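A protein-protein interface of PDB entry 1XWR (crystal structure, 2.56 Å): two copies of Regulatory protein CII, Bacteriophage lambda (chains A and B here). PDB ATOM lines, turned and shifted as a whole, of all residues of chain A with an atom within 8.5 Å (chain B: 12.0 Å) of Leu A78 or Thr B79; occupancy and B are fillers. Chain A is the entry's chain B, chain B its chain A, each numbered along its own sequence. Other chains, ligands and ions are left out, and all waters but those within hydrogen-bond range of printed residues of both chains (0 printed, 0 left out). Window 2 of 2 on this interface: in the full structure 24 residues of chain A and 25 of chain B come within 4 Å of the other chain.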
ATOM      1  N   ALA A  71      29.185 -18.773 -16.576  1.00  0.00           N
ATOM      2  CA  ALA A  71      28.794 -20.148 -16.307  1.00  0.00           C
ATOM      3  C   ALA A  71      29.158 -20.520 -14.879  1.00  0.00           C
ATOM      4  O   ALA A  71      28.350 -21.109 -14.169  1.00  0.00           O
ATOM      5  CB  ALA A  71      29.468 -21.092 -17.284  1.00  0.00           C
ATOM      6  N   ARG A  72      30.376 -20.174 -14.460  1.00  0.00           N
ATOM      7  CA  ARG A  72      30.819 -20.474 -13.099  1.00  0.00           C
ATOM      8  C   ARG A  72      29.875 -19.786 -12.120  1.00  0.00           C
ATOM      9  O   ARG A  72      29.171 -20.447 -11.358  1.00  0.00           O
ATOM     10  CB  ARG A  72      32.245 -19.968 -12.844  1.00  0.00           C
ATOM     11  CG  ARG A  72      33.331 -20.549 -13.743  1.00  0.00           C
ATOM     12  CD  ARG A  72      34.708 -20.318 -13.121  1.00  0.00           C
ATOM     13  NE  ARG A  72      34.833 -18.968 -12.566  1.00  0.00           N
ATOM     14  CZ  ARG A  72      35.120 -17.881 -13.278  1.00  0.00           C
ATOM     15  NH1 ARG A  72      35.328 -17.981 -14.587  1.00  0.00           N
ATOM     16  NH2 ARG A  72      35.179 -16.690 -12.685  1.00  0.00           N
ATOM     17  N   GLN A  73      29.860 -18.455 -12.158  1.00  0.00           N
ATOM     18  CA  GLN A  73      29.007 -17.671 -11.274  1.00  0.00           C
ATOM     19  C   GLN A  73      27.600 -18.253 -11.182  1.00  0.00           C
ATOM     20  O   GLN A  73      27.000 -18.264 -10.109  1.00  0.00           O
ATOM     21  CB  GLN A  73      28.921 -16.214 -11.744  1.00  0.00           C
ATOM     22  CG  GLN A  73      30.236 -15.452 -11.749  1.00  0.00           C
ATOM     23  CD  GLN A  73      30.060 -13.975 -12.116  1.00  0.00           C
ATOM     24  OE1 GLN A  73      31.038 -13.237 -12.279  1.00  0.00           O
ATOM     25  NE2 GLN A  73      28.809 -13.540 -12.241  1.00  0.00           N
ATOM     26  N   VAL A  74      27.070 -18.733 -12.304  1.00  0.00           N
ATOM     27  CA  VAL A  74      25.730 -19.313 -12.322  1.00  0.00           C
ATOM     28  C   VAL A  74      25.747 -20.665 -11.624  1.00  0.00           C
ATOM     29  O   VAL A  74      24.830 -20.999 -10.873  1.00  0.00           O
ATOM     30  CB  VAL A  74      25.206 -19.522 -13.767  1.00  0.00           C
ATOM     31  CG1 VAL A  74      23.877 -20.265 -13.739  1.00  0.00           C
ATOM     32  CG2 VAL A  74      25.028 -18.183 -14.455  1.00  0.00           C
ATOM     33  N   ALA A  75      26.797 -21.437 -11.877  1.00  0.00           N
ATOM     34  CA  ALA A  75      26.937 -22.758 -11.280  1.00  0.00           C
ATOM     35  C   ALA A  75      26.997 -22.649  -9.755  1.00  0.00           C
ATOM     36  O   ALA A  75      26.630 -23.586  -9.041  1.00  0.00           O
ATOM     37  CB  ALA A  75      28.197 -23.447 -11.814  1.00  0.00           C
ATOM     38  N   ALA A  76      27.455 -21.503  -9.259  1.00  0.00           N
ATOM     39  CA  ALA A  76      27.554 -21.287  -7.818  1.00  0.00           C
ATOM     40  C   ALA A  76      26.184 -21.010  -7.202  1.00  0.00           C
ATOM     41  O   ALA A  76      25.738 -21.732  -6.313  1.00  0.00           O
ATOM     42  CB  ALA A  76      28.509 -20.134  -7.521  1.00  0.00           C
ATOM     43  N   ILE A  77      25.513 -19.969  -7.678  1.00  0.00           N
ATOM     44  CA  ILE A  77      24.200 -19.623  -7.155  1.00  0.00           C
ATOM     45  C   ILE A  77      23.219 -20.791  -7.326  1.00  0.00           C
ATOM     46  O   ILE A  77      22.174 -20.836  -6.672  1.00  0.00           O
ATOM     47  CB  ILE A  77      23.645 -18.347  -7.850  1.00  0.00           C
ATOM     48  CG1 ILE A  77      22.279 -17.976  -7.267  1.00  0.00           C
ATOM     49  CG2 ILE A  77      23.558 -18.569  -9.347  1.00  0.00           C
ATOM     50  CD1 ILE A  77      21.721 -16.652  -7.772  1.00  0.00           C
ATOM     51  N   LEU A  78      23.564 -21.742  -8.190  1.00  0.00           N
ATOM     52  CA  LEU A  78      22.700 -22.896  -8.422  1.00  0.00           C
ATOM     53  C   LEU A  78      22.864 -24.001  -7.386  1.00  0.00           C
ATOM     54  O   LEU A  78      21.932 -24.772  -7.147  1.00  0.00           O
ATOM     55  CB  LEU A  78      22.933 -23.490  -9.815  1.00  0.00           C
ATOM     56  CG  LEU A  78      22.064 -22.962 -10.959  1.00  0.00           C
ATOM     57  CD1 LEU A  78      22.275 -23.835 -12.186  1.00  0.00           C
ATOM     58  CD2 LEU A  78      20.596 -22.981 -10.555  1.00  0.00           C
ATOM     59  N   THR A  79      24.044 -24.085  -6.776  1.00  0.00           N
ATOM     60  CA  THR A  79      24.298 -25.116  -5.770  1.00  0.00           C
ATOM     61  C   THR A  79      23.844 -24.687  -4.367  1.00  0.00           C
ATOM     62  O   THR A  79      23.218 -25.469  -3.639  1.00  0.00           O
ATOM     63  CB  THR A  79      25.801 -25.506  -5.726  1.00  0.00           C
ATOM     64  OG1 THR A  79      26.593 -24.360  -5.386  1.00  0.00           O
ATOM     65  CG2 THR A  79      26.249 -26.054  -7.080  1.00  0.00           C
ATOM     66  N   ASN A  80      24.151 -23.447  -3.996  1.00  0.00           N
ATOM     67  CA  ASN A  80      23.771 -22.929  -2.686  1.00  0.00           C
ATOM     68  C   ASN A  80      22.262 -22.668  -2.607  1.00  0.00           C
ATOM     69  O   ASN A  80      21.878 -21.570  -2.144  1.00  0.00           O
ATOM     70  CB  ASN A  80      24.542 -21.636  -2.391  1.00  0.00           C
ATOM     71  CG  ASN A  80      26.051 -21.834  -2.396  1.00  0.00           C
ATOM     72  OD1 ASN A  80      26.582 -22.656  -1.653  1.00  0.00           O
ATOM     73  ND2 ASN A  80      26.745 -21.074  -3.234  1.00  0.00           N
ATOM     74  N   MET B  67      27.299  -8.689 -14.597  1.00  0.00           N
ATOM     75  CA  MET B  67      27.551 -10.122 -14.588  1.00  0.00           C
ATOM     76  C   MET B  67      26.757 -10.802 -13.479  1.00  0.00           C
ATOM     77  O   MET B  67      26.122 -11.837 -13.706  1.00  0.00           O
ATOM     78  CB  MET B  67      29.040 -10.391 -14.395  1.00  0.00           C
ATOM     79  CG  MET B  67      29.837 -10.194 -15.659  1.00  0.00           C
ATOM     80  SD  MET B  67      29.281 -11.340 -16.942  1.00  0.00           S
ATOM     81  CE  MET B  67      30.543 -12.625 -16.808  1.00  0.00           C
ATOM     82  N   ALA B  68      26.793 -10.214 -12.283  1.00  0.00           N
ATOM     83  CA  ALA B  68      26.071 -10.765 -11.145  1.00  0.00           C
ATOM     84  C   ALA B  68      24.579 -10.829 -11.468  1.00  0.00           C
ATOM     85  O   ALA B  68      23.932 -11.853 -11.238  1.00  0.00           O
ATOM     86  CB  ALA B  68      26.312  -9.921  -9.898  1.00  0.00           C
ATOM     87  N   ARG B  69      24.037  -9.741 -12.009  1.00  0.00           N
ATOM     88  CA  ARG B  69      22.626  -9.703 -12.366  1.00  0.00           C
ATOM     89  C   ARG B  69      22.309 -10.802 -13.378  1.00  0.00           C
ATOM     90  O   ARG B  69      21.306 -11.508 -13.258  1.00  0.00           O
ATOM     91  CB  ARG B  69      22.271  -8.348 -12.970  1.00  0.00           C
ATOM     92  CG  ARG B  69      20.812  -8.223 -13.377  1.00  0.00           C
ATOM     93  CD  ARG B  69      20.589  -7.054 -14.342  1.00  0.00           C
ATOM     94  NE  ARG B  69      21.223  -7.295 -15.641  1.00  0.00           N
ATOM     95  CZ  ARG B  69      22.127  -6.495 -16.205  1.00  0.00           C
ATOM     96  NH1 ARG B  69      22.513  -5.379 -15.589  1.00  0.00           N
ATOM     97  NH2 ARG B  69      22.657  -6.821 -17.382  1.00  0.00           N
ATOM     98  N   LEU B  70      23.173 -10.931 -14.381  1.00  0.00           N
ATOM     99  CA  LEU B  70      23.013 -11.936 -15.426  1.00  0.00           C
ATOM    100  C   LEU B  70      23.064 -13.332 -14.826  1.00  0.00           C
ATOM    101  O   LEU B  70      22.286 -14.203 -15.198  1.00  0.00           O
ATOM    102  CB  LEU B  70      24.132 -11.791 -16.461  1.00  0.00           C
ATOM    103  CG  LEU B  70      23.786 -11.235 -17.842  1.00  0.00           C
ATOM    104  CD1 LEU B  70      22.755 -10.128 -17.747  1.00  0.00           C
ATOM    105  CD2 LEU B  70      25.071 -10.742 -18.488  1.00  0.00           C
ATOM    106  N   ALA B  71      23.993 -13.544 -13.902  1.00  0.00           N
ATOM    107  CA  ALA B  71      24.131 -14.842 -13.262  1.00  0.00           C
ATOM    108  C   ALA B  71      22.839 -15.211 -12.537  1.00  0.00           C
ATOM    109  O   ALA B  71      22.342 -16.333 -12.646  1.00  0.00           O
ATOM    110  CB  ALA B  71      25.290 -14.821 -12.278  1.00  0.00           C
ATOM    111  N   ARG B  72      22.291 -14.262 -11.798  1.00  0.00           N
ATOM    112  CA  ARG B  72      21.064 -14.523 -11.076  1.00  0.00           C
ATOM    113  C   ARG B  72      19.922 -14.814 -12.047  1.00  0.00           C
ATOM    114  O   ARG B  72      19.224 -15.817 -11.905  1.00  0.00           O
ATOM    115  CB  ARG B  72      20.731 -13.335 -10.149  1.00  0.00           C
ATOM    116  CG  ARG B  72      21.786 -13.125  -9.040  1.00  0.00           C
ATOM    117  CD  ARG B  72      21.427 -12.060  -7.979  1.00  0.00           C
ATOM    118  NE  ARG B  72      21.615 -10.670  -8.415  1.00  0.00           N
ATOM    119  CZ  ARG B  72      20.677  -9.929  -9.008  1.00  0.00           C
ATOM    120  NH1 ARG B  72      19.467 -10.436  -9.245  1.00  0.00           N
ATOM    121  NH2 ARG B  72      20.945  -8.675  -9.358  1.00  0.00           N
ATOM    122  N   GLN B  73      19.740 -13.953 -13.042  1.00  0.00           N
ATOM    123  CA  GLN B  73      18.674 -14.154 -14.018  1.00  0.00           C
ATOM    124  C   GLN B  73      18.794 -15.507 -14.703  1.00  0.00           C
ATOM    125  O   GLN B  73      17.794 -16.175 -14.929  1.00  0.00           O
ATOM    126  CB  GLN B  73      18.705 -13.041 -15.062  1.00  0.00           C
ATOM    127  CG  GLN B  73      18.380 -11.680 -14.487  1.00  0.00           C
ATOM    128  CD  GLN B  73      18.552 -10.551 -15.486  1.00  0.00           C
ATOM    129  OE1 GLN B  73      18.260  -9.394 -15.181  1.00  0.00           O
ATOM    130  NE2 GLN B  73      19.033 -10.877 -16.683  1.00  0.00           N
ATOM    131  N   VAL B  74      20.016 -15.917 -15.029  1.00  0.00           N
ATOM    132  CA  VAL B  74      20.219 -17.199 -15.687  1.00  0.00           C
ATOM    133  C   VAL B  74      19.945 -18.341 -14.731  1.00  0.00           C
ATOM    134  O   VAL B  74      19.283 -19.315 -15.097  1.00  0.00           O
ATOM    135  CB  VAL B  74      21.641 -17.352 -16.243  1.00  0.00           C
ATOM    136  CG1 VAL B  74      21.842 -18.763 -16.780  1.00  0.00           C
ATOM    137  CG2 VAL B  74      21.858 -16.351 -17.350  1.00  0.00           C
ATOM    138  N   ALA B  75      20.461 -18.214 -13.511  1.00  0.00           N
ATOM    139  CA  ALA B  75      20.268 -19.224 -12.478  1.00  0.00           C
ATOM    140  C   ALA B  75      18.777 -19.504 -12.308  1.00  0.00           C
ATOM    141  O   ALA B  75      18.352 -20.657 -12.228  1.00  0.00           O
ATOM    142  CB  ALA B  75      20.867 -18.742 -11.177  1.00  0.00           C
ATOM    143  N   ALA B  76      17.986 -18.437 -12.273  1.00  0.00           N
ATOM    144  CA  ALA B  76      16.542 -18.552 -12.122  1.00  0.00           C
ATOM    145  C   ALA B  76      15.908 -19.378 -13.236  1.00  0.00           C
ATOM    146  O   ALA B  76      15.041 -20.204 -12.982  1.00  0.00           O
ATOM    147  CB  ALA B  76      15.910 -17.164 -12.081  1.00  0.00           C
ATOM    148  N   ILE B  77      16.334 -19.158 -14.474  1.00  0.00           N
ATOM    149  CA  ILE B  77      15.763 -19.899 -15.589  1.00  0.00           C
ATOM    150  C   ILE B  77      16.222 -21.346 -15.576  1.00  0.00           C
ATOM    151  O   ILE B  77      15.529 -22.226 -16.077  1.00  0.00           O
ATOM    152  CB  ILE B  77      16.155 -19.291 -16.947  1.00  0.00           C
ATOM    153  CG1 ILE B  77      15.852 -17.795 -16.965  1.00  0.00           C
ATOM    154  CG2 ILE B  77      15.362 -19.950 -18.044  1.00  0.00           C
ATOM    155  CD1 ILE B  77      16.150 -17.130 -18.287  1.00  0.00           C
ATOM    156  N   LEU B  78      17.388 -21.595 -14.997  1.00  0.00           N
ATOM    157  CA  LEU B  78      17.910 -22.946 -14.958  1.00  0.00           C
ATOM    158  C   LEU B  78      17.551 -23.749 -13.709  1.00  0.00           C
ATOM    159  O   LEU B  78      18.154 -24.792 -13.449  1.00  0.00           O
ATOM    160  CB  LEU B  78      19.422 -22.913 -15.139  1.00  0.00           C
ATOM    161  CG  LEU B  78      19.820 -22.462 -16.541  1.00  0.00           C
ATOM    162  CD1 LEU B  78      21.329 -22.351 -16.632  1.00  0.00           C
ATOM    163  CD2 LEU B  78      19.275 -23.454 -17.562  1.00  0.00           C
ATOM    164  N   THR B  79      16.580 -23.270 -12.934  1.00  0.00           N
ATOM    165  CA  THR B  79      16.152 -23.995 -11.734  1.00  0.00           C
ATOM    166  C   THR B  79      14.781 -24.629 -11.974  1.00  0.00           C
ATOM    167  O   THR B  79      14.012 -24.172 -12.824  1.00  0.00           O
ATOM    168  CB  THR B  79      16.080 -23.078 -10.479  1.00  0.00           C
ATOM    169  OG1 THR B  79      15.180 -21.990 -10.723  1.00  0.00           O
ATOM    170  CG2 THR B  79      17.459 -22.538 -10.128  1.00  0.00           C
ATOM    171  N   ASN B  80      14.485 -25.682 -11.217  1.00  0.00           N
ATOM    172  CA  ASN B  80      13.228 -26.416 -11.346  1.00  0.00           C
ATOM    173  C   ASN B  80      12.012 -25.781 -10.672  1.00  0.00           C
ATOM    174  O   ASN B  80      11.977 -25.773  -9.423  1.00  0.00           O
ATOM    175  CB  ASN B  80      13.431 -27.837 -10.828  1.00  0.00           C
ATOM    176  CG  ASN B  80      14.438 -28.601 -11.653  1.00  0.00           C
ATOM    177  OD1 ASN B  80      14.174 -28.941 -12.809  1.00  0.00           O
ATOM    178  ND2 ASN B  80      15.609 -28.860 -11.075  1.00  0.00           N
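O of Ala B76 sits at hydrogen-bond distance from OG1 of Thr B79 (2.9 Å).
Met B67 touches Gln A73.
Gln A73 touches Ala B68 (NE2 to N, 3.9 Å).
Gln A73 touches Ala B71.
Val A74 touches Ala B71.
Val A74 touches Val B74.
Val A74 touches Ala B75 (CG1 to CA, 3.96 Å).
CD1 of Ile A77 touches CG of Arg B72 (3.7 Å).
CB of Ala B75 touches CG2 of Ile A77 (3.3 Å).
Ala B75 touches Leu A78 (O to CD2, 3.6 Å).
Leu A78 touches Thr B79 (CD2 to CG2, 3.2 Å).
Val A74 touches just these residues of chain B: Ala B71 (3.7 Å), Val B74 (3.9 Å) and Ala B75 (3.96 Å).
No residue of chain B comes within 4 Å of Ala A76.
Ile A77 touches just these residues of chain B: Arg B72 (3.7 Å) and Ala B75 (3.3 Å).
No residue of chain B comes within 4 Å of Thr A79.
Of the printed residues of chain A, Met B67 touches Gln A73.
Of the printed residues of chain A, Ala B68 touches Gln A73 (3.9 Å).
Of the printed residues of chain A, Ala B75 touches Val A74, Ile A77 and Leu A78.
Leu B78 touches none of the printed residues of chain A.
Thr B79 touches one residue of chain A.
No residue of chain A comes within 4 Å of Asn B80.
The nearest residue of chain B that does not touch Leu A78 is Leu B78 (4.2 Å).
Hydrophobic or aromatic side chains of chain B within 4 Å of the printed part of chain A: Met B67, Ala B71, Val B74 and Ala B75.
Among the printed residues, 10 pairs touch across the chains.
Among the printed residues, no Asp or Glu carboxylate lies within 4 Å of a Lys or Arg side-chain nitrogen of the other chain.
Gln A73 touches Ala B71, but with the chains exchanged Ala A71 does not touch Gln B73 (11.1 Å).
Val B74 touches its own counterpart, Val A74.
Ile A77 touches Ala B75, but with the chains exchanged Ala A75 does not touch Ile B77 (11.0 Å).
Leu A78 touches Thr B79, but with the chains exchanged Thr A79 does not touch Leu B78 (8.9 Å).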
